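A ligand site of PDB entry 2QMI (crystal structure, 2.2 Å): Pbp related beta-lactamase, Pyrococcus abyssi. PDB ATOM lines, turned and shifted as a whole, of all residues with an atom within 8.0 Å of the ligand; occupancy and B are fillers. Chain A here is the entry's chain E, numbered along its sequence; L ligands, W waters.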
ATOM      1  N   SER A  79     -30.365  -4.174  -7.670  1.00  0.00           N
ATOM      2  CA  SER A  79     -29.205  -3.751  -6.890  1.00  0.00           C
ATOM      3  C   SER A  79     -27.942  -4.372  -7.490  1.00  0.00           C
ATOM      4  O   SER A  79     -27.976  -5.486  -8.012  1.00  0.00           O
ATOM      5  CB  SER A  79     -29.342  -4.187  -5.428  1.00  0.00           C
ATOM      6  OG  SER A  79     -28.135  -3.941  -4.723  1.00  0.00           O
ATOM      7  N   LEU A  80     -26.831  -3.656  -7.408  1.00  0.00           N
ATOM      8  CA  LEU A  80     -25.579  -4.156  -7.945  1.00  0.00           C
ATOM      9  C   LEU A  80     -25.111  -5.387  -7.185  1.00  0.00           C
ATOM     10  O   LEU A  80     -24.367  -6.196  -7.724  1.00  0.00           O
ATOM     11  CB  LEU A  80     -24.515  -3.058  -7.907  1.00  0.00           C
ATOM     12  CG  LEU A  80     -24.757  -1.896  -8.869  1.00  0.00           C
ATOM     13  CD1 LEU A  80     -23.889  -0.710  -8.500  1.00  0.00           C
ATOM     14  CD2 LEU A  80     -24.483  -2.349 -10.286  1.00  0.00           C
ATOM     15  N   ASP A  81     -25.561  -5.542  -5.936  1.00  0.00           N
ATOM     16  CA  ASP A  81     -25.180  -6.696  -5.134  1.00  0.00           C
ATOM     17  C   ASP A  81     -26.178  -7.853  -5.228  1.00  0.00           C
ATOM     18  O   ASP A  81     -26.074  -8.834  -4.480  1.00  0.00           O
ATOM     19  CB  ASP A  81     -25.014  -6.306  -3.669  1.00  0.00           C
ATOM     20  CG  ASP A  81     -23.926  -5.276  -3.457  1.00  0.00           C
ATOM     21  OD1 ASP A  81     -22.793  -5.491  -3.920  1.00  0.00           O
ATOM     22  OD2 ASP A  81     -24.206  -4.223  -2.835  1.00  0.00           O
ATOM     23  N   ASP A  82     -27.156  -7.738  -6.126  1.00  0.00           N
ATOM     24  CA  ASP A  82     -28.142  -8.807  -6.305  1.00  0.00           C
ATOM     25  C   ASP A  82     -27.553 -10.027  -6.979  1.00  0.00           C
ATOM     26  O   ASP A  82     -26.806  -9.916  -7.951  1.00  0.00           O
ATOM     27  CB  ASP A  82     -29.318  -8.353  -7.172  1.00  0.00           C
ATOM     28  CG  ASP A  82     -30.400  -7.644  -6.388  1.00  0.00           C
ATOM     29  OD1 ASP A  82     -30.506  -7.873  -5.162  1.00  0.00           O
ATOM     30  OD2 ASP A  82     -31.143  -6.870  -7.018  1.00  0.00           O
ATOM     31  N   THR A 100     -22.845 -11.984  -8.125  1.00  0.00           N
ATOM     32  CA  THR A 100     -23.722 -10.815  -8.155  1.00  0.00           C
ATOM     33  C   THR A 100     -23.618 -10.042  -9.466  1.00  0.00           C
ATOM     34  O   THR A 100     -22.749 -10.326 -10.291  1.00  0.00           O
ATOM     35  CB  THR A 100     -23.395  -9.817  -6.992  1.00  0.00           C
ATOM     36  OG1 THR A 100     -22.143  -9.179  -7.244  1.00  0.00           O
ATOM     37  CG2 THR A 100     -23.321 -10.560  -5.667  1.00  0.00           C
ATOM     38  N   VAL A 101     -24.491  -9.063  -9.659  1.00  0.00           N
ATOM     39  CA  VAL A 101     -24.477  -8.237 -10.858  1.00  0.00           C
ATOM     40  C   VAL A 101     -23.120  -7.534 -10.931  1.00  0.00           C
ATOM     41  O   VAL A 101     -22.542  -7.388 -12.008  1.00  0.00           O
ATOM     42  CB  VAL A 101     -25.592  -7.147 -10.802  1.00  0.00           C
ATOM     43  CG1 VAL A 101     -25.346  -6.103 -11.883  1.00  0.00           C
ATOM     44  CG2 VAL A 101     -26.966  -7.789 -10.997  1.00  0.00           C
ATOM     45  N   HIS A 102     -22.638  -7.107  -9.771  1.00  0.00           N
ATOM     46  CA  HIS A 102     -21.362  -6.410  -9.657  1.00  0.00           C
ATOM     47  C   HIS A 102     -20.212  -7.296 -10.149  1.00  0.00           C
ATOM     48  O   HIS A 102     -19.320  -6.831 -10.854  1.00  0.00           O
ATOM     49  CB  HIS A 102     -21.129  -5.996  -8.200  1.00  0.00           C
ATOM     50  CG  HIS A 102     -19.840  -5.291  -7.964  1.00  0.00           C
ATOM     51  ND1 HIS A 102     -19.636  -3.978  -8.327  1.00  0.00           N
ATOM     52  CD2 HIS A 102     -18.669  -5.716  -7.431  1.00  0.00           C
ATOM     53  CE1 HIS A 102     -18.392  -3.626  -8.035  1.00  0.00           C
ATOM     54  NE2 HIS A 102     -17.786  -4.668  -7.485  1.00  0.00           N
ATOM     55  N   HIS A 103     -20.241  -8.564  -9.770  1.00  0.00           N
ATOM     56  CA  HIS A 103     -19.206  -9.509 -10.180  1.00  0.00           C
ATOM     57  C   HIS A 103     -19.134  -9.657 -11.700  1.00  0.00           C
ATOM     58  O   HIS A 103     -18.048  -9.730 -12.264  1.00  0.00           O
ATOM     59  CB  HIS A 103     -19.426 -10.875  -9.545  1.00  0.00           C
ATOM     60  CG  HIS A 103     -19.358 -10.867  -8.055  1.00  0.00           C
ATOM     61  ND1 HIS A 103     -18.352 -10.242  -7.354  1.00  0.00           N
ATOM     62  CD2 HIS A 103     -20.141 -11.462  -7.123  1.00  0.00           C
ATOM     63  CE1 HIS A 103     -18.516 -10.434  -6.064  1.00  0.00           C
ATOM     64  NE2 HIS A 103     -19.597 -11.177  -5.889  1.00  0.00           N
ATOM     65  N   LEU A 105     -20.142  -7.448 -14.017  1.00  0.00           N
ATOM     66  CA  LEU A 105     -19.666  -6.165 -14.532  1.00  0.00           C
ATOM     67  C   LEU A 105     -18.137  -6.058 -14.503  1.00  0.00           C
ATOM     68  O   LEU A 105     -17.521  -5.508 -15.428  1.00  0.00           O
ATOM     69  CB  LEU A 105     -20.262  -5.027 -13.697  1.00  0.00           C
ATOM     70  CG  LEU A 105     -21.358  -4.063 -14.199  1.00  0.00           C
ATOM     71  CD1 LEU A 105     -21.964  -4.511 -15.524  1.00  0.00           C
ATOM     72  CD2 LEU A 105     -22.435  -3.954 -13.118  1.00  0.00           C
ATOM     73  N   THR A 106     -17.522  -6.573 -13.447  1.00  0.00           N
ATOM     74  CA  THR A 106     -16.078  -6.509 -13.291  1.00  0.00           C
ATOM     75  C   THR A 106     -15.302  -7.754 -13.685  1.00  0.00           C
ATOM     76  O   THR A 106     -14.090  -7.820 -13.483  1.00  0.00           O
ATOM     77  CB  THR A 106     -15.699  -6.151 -11.836  1.00  0.00           C
ATOM     78  OG1 THR A 106     -16.281  -7.099 -10.937  1.00  0.00           O
ATOM     79  CG2 THR A 106     -16.195  -4.744 -11.491  1.00  0.00           C
ATOM     80  N   SER A 108     -15.315 -10.686 -12.345  1.00  0.00           N
ATOM     81  CA  SER A 108     -14.747 -11.274 -11.147  1.00  0.00           C
ATOM     82  C   SER A 108     -15.616 -12.359 -10.525  1.00  0.00           C
ATOM     83  O   SER A 108     -15.543 -12.602  -9.336  1.00  0.00           O
ATOM     84  CB  SER A 108     -14.487 -10.166 -10.098  1.00  0.00           C
ATOM     85  OG  SER A 108     -15.699  -9.561  -9.677  1.00  0.00           O
ATOM     86  N   GLY A 155     -15.286 -12.382  -6.705  1.00  0.00           N
ATOM     87  CA  GLY A 155     -14.612 -11.176  -6.259  1.00  0.00           C
ATOM     88  C   GLY A 155     -13.128 -11.249  -5.940  1.00  0.00           C
ATOM     89  O   GLY A 155     -12.553 -10.243  -5.519  1.00  0.00           O
ATOM     90  N   LYS A 266     -19.219   5.787 -11.089  1.00  0.00           N
ATOM     91  CA  LYS A 266     -19.219   4.408 -10.596  1.00  0.00           C
ATOM     92  C   LYS A 266     -18.583   3.523 -11.677  1.00  0.00           C
ATOM     93  O   LYS A 266     -17.763   2.664 -11.381  1.00  0.00           O
ATOM     94  CB  LYS A 266     -20.646   3.911 -10.323  1.00  0.00           C
ATOM     95  CG  LYS A 266     -21.237   4.349  -8.988  1.00  0.00           C
ATOM     96  CD  LYS A 266     -22.674   3.830  -8.839  1.00  0.00           C
ATOM     97  CE  LYS A 266     -23.413   4.461  -7.667  1.00  0.00           C
ATOM     98  NZ  LYS A 266     -22.940   4.011  -6.342  1.00  0.00           N
ATOM     99  N   THR A 269     -14.724   3.753 -11.898  1.00  0.00           N
ATOM    100  CA  THR A 269     -13.975   3.409 -10.697  1.00  0.00           C
ATOM    101  C   THR A 269     -13.249   2.078 -10.909  1.00  0.00           C
ATOM    102  O   THR A 269     -13.846   1.107 -11.351  1.00  0.00           O
ATOM    103  CB  THR A 269     -14.910   3.306  -9.490  1.00  0.00           C
ATOM    104  OG1 THR A 269     -15.549   4.568  -9.277  1.00  0.00           O
ATOM    105  CG2 THR A 269     -14.142   2.930  -8.236  1.00  0.00           C
ATOM    106  N   SER A 270     -11.961   2.057 -10.592  1.00  0.00           N
ATOM    107  CA  SER A 270     -11.163   0.844 -10.741  1.00  0.00           C
ATOM    108  C   SER A 270     -11.468  -0.108  -9.574  1.00  0.00           C
ATOM    109  O   SER A 270     -10.991   0.107  -8.468  1.00  0.00           O
ATOM    110  CB  SER A 270      -9.672   1.188 -10.750  1.00  0.00           C
ATOM    111  OG  SER A 270      -8.867   0.031 -10.928  1.00  0.00           O
ATOM    112  N   TYR A 271     -12.251  -1.151  -9.839  1.00  0.00           N
ATOM    113  CA  TYR A 271     -12.635  -2.123  -8.815  1.00  0.00           C
ATOM    114  C   TYR A 271     -11.661  -3.281  -8.649  1.00  0.00           C
ATOM    115  O   TYR A 271     -11.542  -3.851  -7.564  1.00  0.00           O
ATOM    116  CB  TYR A 271     -14.031  -2.697  -9.119  1.00  0.00           C
ATOM    117  CG  TYR A 271     -15.140  -1.658  -9.103  1.00  0.00           C
ATOM    118  CD1 TYR A 271     -15.669  -1.196  -7.905  1.00  0.00           C
ATOM    119  CD2 TYR A 271     -15.609  -1.085 -10.297  1.00  0.00           C
ATOM    120  CE1 TYR A 271     -16.659  -0.198  -7.884  1.00  0.00           C
ATOM    121  CE2 TYR A 271     -16.583  -0.083 -10.282  1.00  0.00           C
ATOM    122  CZ  TYR A 271     -17.104   0.358  -9.075  1.00  0.00           C
ATOM    123  OH  TYR A 271     -18.051   1.365  -9.051  1.00  0.00           O
ATOM    124  N   TYR A 286     -16.723  -0.654 -14.862  1.00  0.00           N
ATOM    125  CA  TYR A 286     -17.941  -1.279 -15.369  1.00  0.00           C
ATOM    126  C   TYR A 286     -17.961  -1.190 -16.900  1.00  0.00           C
ATOM    127  O   TYR A 286     -18.408  -0.191 -17.477  1.00  0.00           O
ATOM    128  CB  TYR A 286     -19.195  -0.600 -14.808  1.00  0.00           C
ATOM    129  CG  TYR A 286     -19.454  -0.858 -13.346  1.00  0.00           C
ATOM    130  CD1 TYR A 286     -18.961  -2.009 -12.711  1.00  0.00           C
ATOM    131  CD2 TYR A 286     -20.233   0.017 -12.592  1.00  0.00           C
ATOM    132  CE1 TYR A 286     -19.262  -2.282 -11.369  1.00  0.00           C
ATOM    133  CE2 TYR A 286     -20.537  -0.242 -11.248  1.00  0.00           C
ATOM    134  CZ  TYR A 286     -20.046  -1.388 -10.656  1.00  0.00           C
ATOM    135  OH  TYR A 286     -20.358  -1.646  -9.335  1.00  0.00           O
HETATM  136  N1  LIG L   1     -18.363  -3.481   0.299  1.00  0.00           N
HETATM  137  N2  LIG L   1     -18.514  -4.957  -2.314  1.00  0.00           N
HETATM  138  N3  LIG L   1     -18.161  -2.530  -3.846  1.00  0.00           N
HETATM  139  N4  LIG L   1     -18.100  -0.962  -1.526  1.00  0.00           N
HETATM  140  O1  LIG L   1     -20.597  -1.855   0.736  1.00  0.00           O
HETATM  141  O2  LIG L   1     -21.152  -4.646  -1.168  1.00  0.00           O
HETATM  142  O3  LIG L   1     -20.949  -3.203  -3.737  1.00  0.00           O
HETATM  143  O4  LIG L   1     -20.955  -0.288  -1.777  1.00  0.00           O
HETATM  144  C1  LIG L   1     -17.609  -4.761   0.136  1.00  0.00           C
HETATM  145  C2  LIG L   1     -17.360  -5.181  -1.292  1.00  0.00           C
HETATM  146  C3  LIG L   1     -17.898  -5.004  -3.639  1.00  0.00           C
HETATM  147  C4  LIG L   1     -17.510  -3.685  -4.299  1.00  0.00           C
HETATM  148  C5  LIG L   1     -17.118  -1.505  -3.680  1.00  0.00           C
HETATM  149  C6  LIG L   1     -16.896  -0.950  -2.315  1.00  0.00           C
HETATM  150  C7  LIG L   1     -17.641  -1.042  -0.102  1.00  0.00           C
HETATM  151  C8  LIG L   1     -17.336  -2.459   0.470  1.00  0.00           C
HETATM  152  C9  LIG L   1     -20.370  -2.669   1.688  1.00  0.00           C
HETATM  153  C10 LIG L   1     -19.186  -3.597   1.514  1.00  0.00           C
HETATM  154  C11 LIG L   1     -20.686  -5.840  -1.301  1.00  0.00           C
HETATM  155  C12 LIG L   1     -19.527  -6.073  -2.193  1.00  0.00           C
HETATM  156  C13 LIG L   1     -20.544  -2.748  -4.846  1.00  0.00           C
HETATM  157  C14 LIG L   1     -19.171  -2.079  -4.857  1.00  0.00           C
HETATM  158  C15 LIG L   1     -20.077   0.590  -1.264  1.00  0.00           C
HETATM  159  C16 LIG L   1     -18.828   0.318  -1.873  1.00  0.00           C
HETATM  160  C17 LIG L   1     -20.513   1.918  -1.541  1.00  0.00           C
HETATM  161  O5  LIG L   1     -21.028  -2.729   2.706  1.00  0.00           O
HETATM  162  O6  LIG L   1     -21.159  -6.819  -0.705  1.00  0.00           O
HETATM  163  O7  LIG L   1     -21.167  -2.806  -5.888  1.00  0.00           O
HETATM  164  O   HOH W   1     -14.656   0.765  -4.204  1.00  0.00           O
HETATM  165  O   HOH W   2     -22.744   0.097  -3.803  1.00  0.00           O
HETATM  166  O   HOH W   3     -21.122  -8.850  -2.622  1.00  0.00           O
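Leu 80 touches the ligand. OH of Tyr 286 touches O7 of the ligand (3.7 Å). Hydrophobic or aromatic side chains that line the ligand: Leu 80 and His 102. The nearest printed residue that does not touch the ligand is Tyr 271 (4.4 Å).
The backbone NH of Asp 81 lies close to the side-chain hydroxyl of Ser 79, at 3.3 Å. A ring nitrogen (ND1) of His 102 is in hydrogen-bond range of the side-chain hydroxyl (OH) of Tyr 286. The backbone NH (N) of His 102 sits at hydrogen-bond distance from the backbone carbonyl oxygen (O) of Leu 80, at 2.8 Å. N of His 102 sits close to OG1 of Thr 100 (3.3 Å). The side-chain hydroxyl (OG1) of Thr 106 is in hydrogen-bond range of the backbone carbonyl oxygen (O) of His 102 (3.1 Å). The backbone carbonyl oxygen of Leu 80 sits close to the backbone NH of Val 101, 3.5 Å away.
An oxygen (O3) of the ligand sits close to the side-chain carboxylate (OD1) of Asp 81 (2.9 Å). An oxygen (O7) of the ligand is in hydrogen-bond range of a ring nitrogen (ND1) of His 102.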
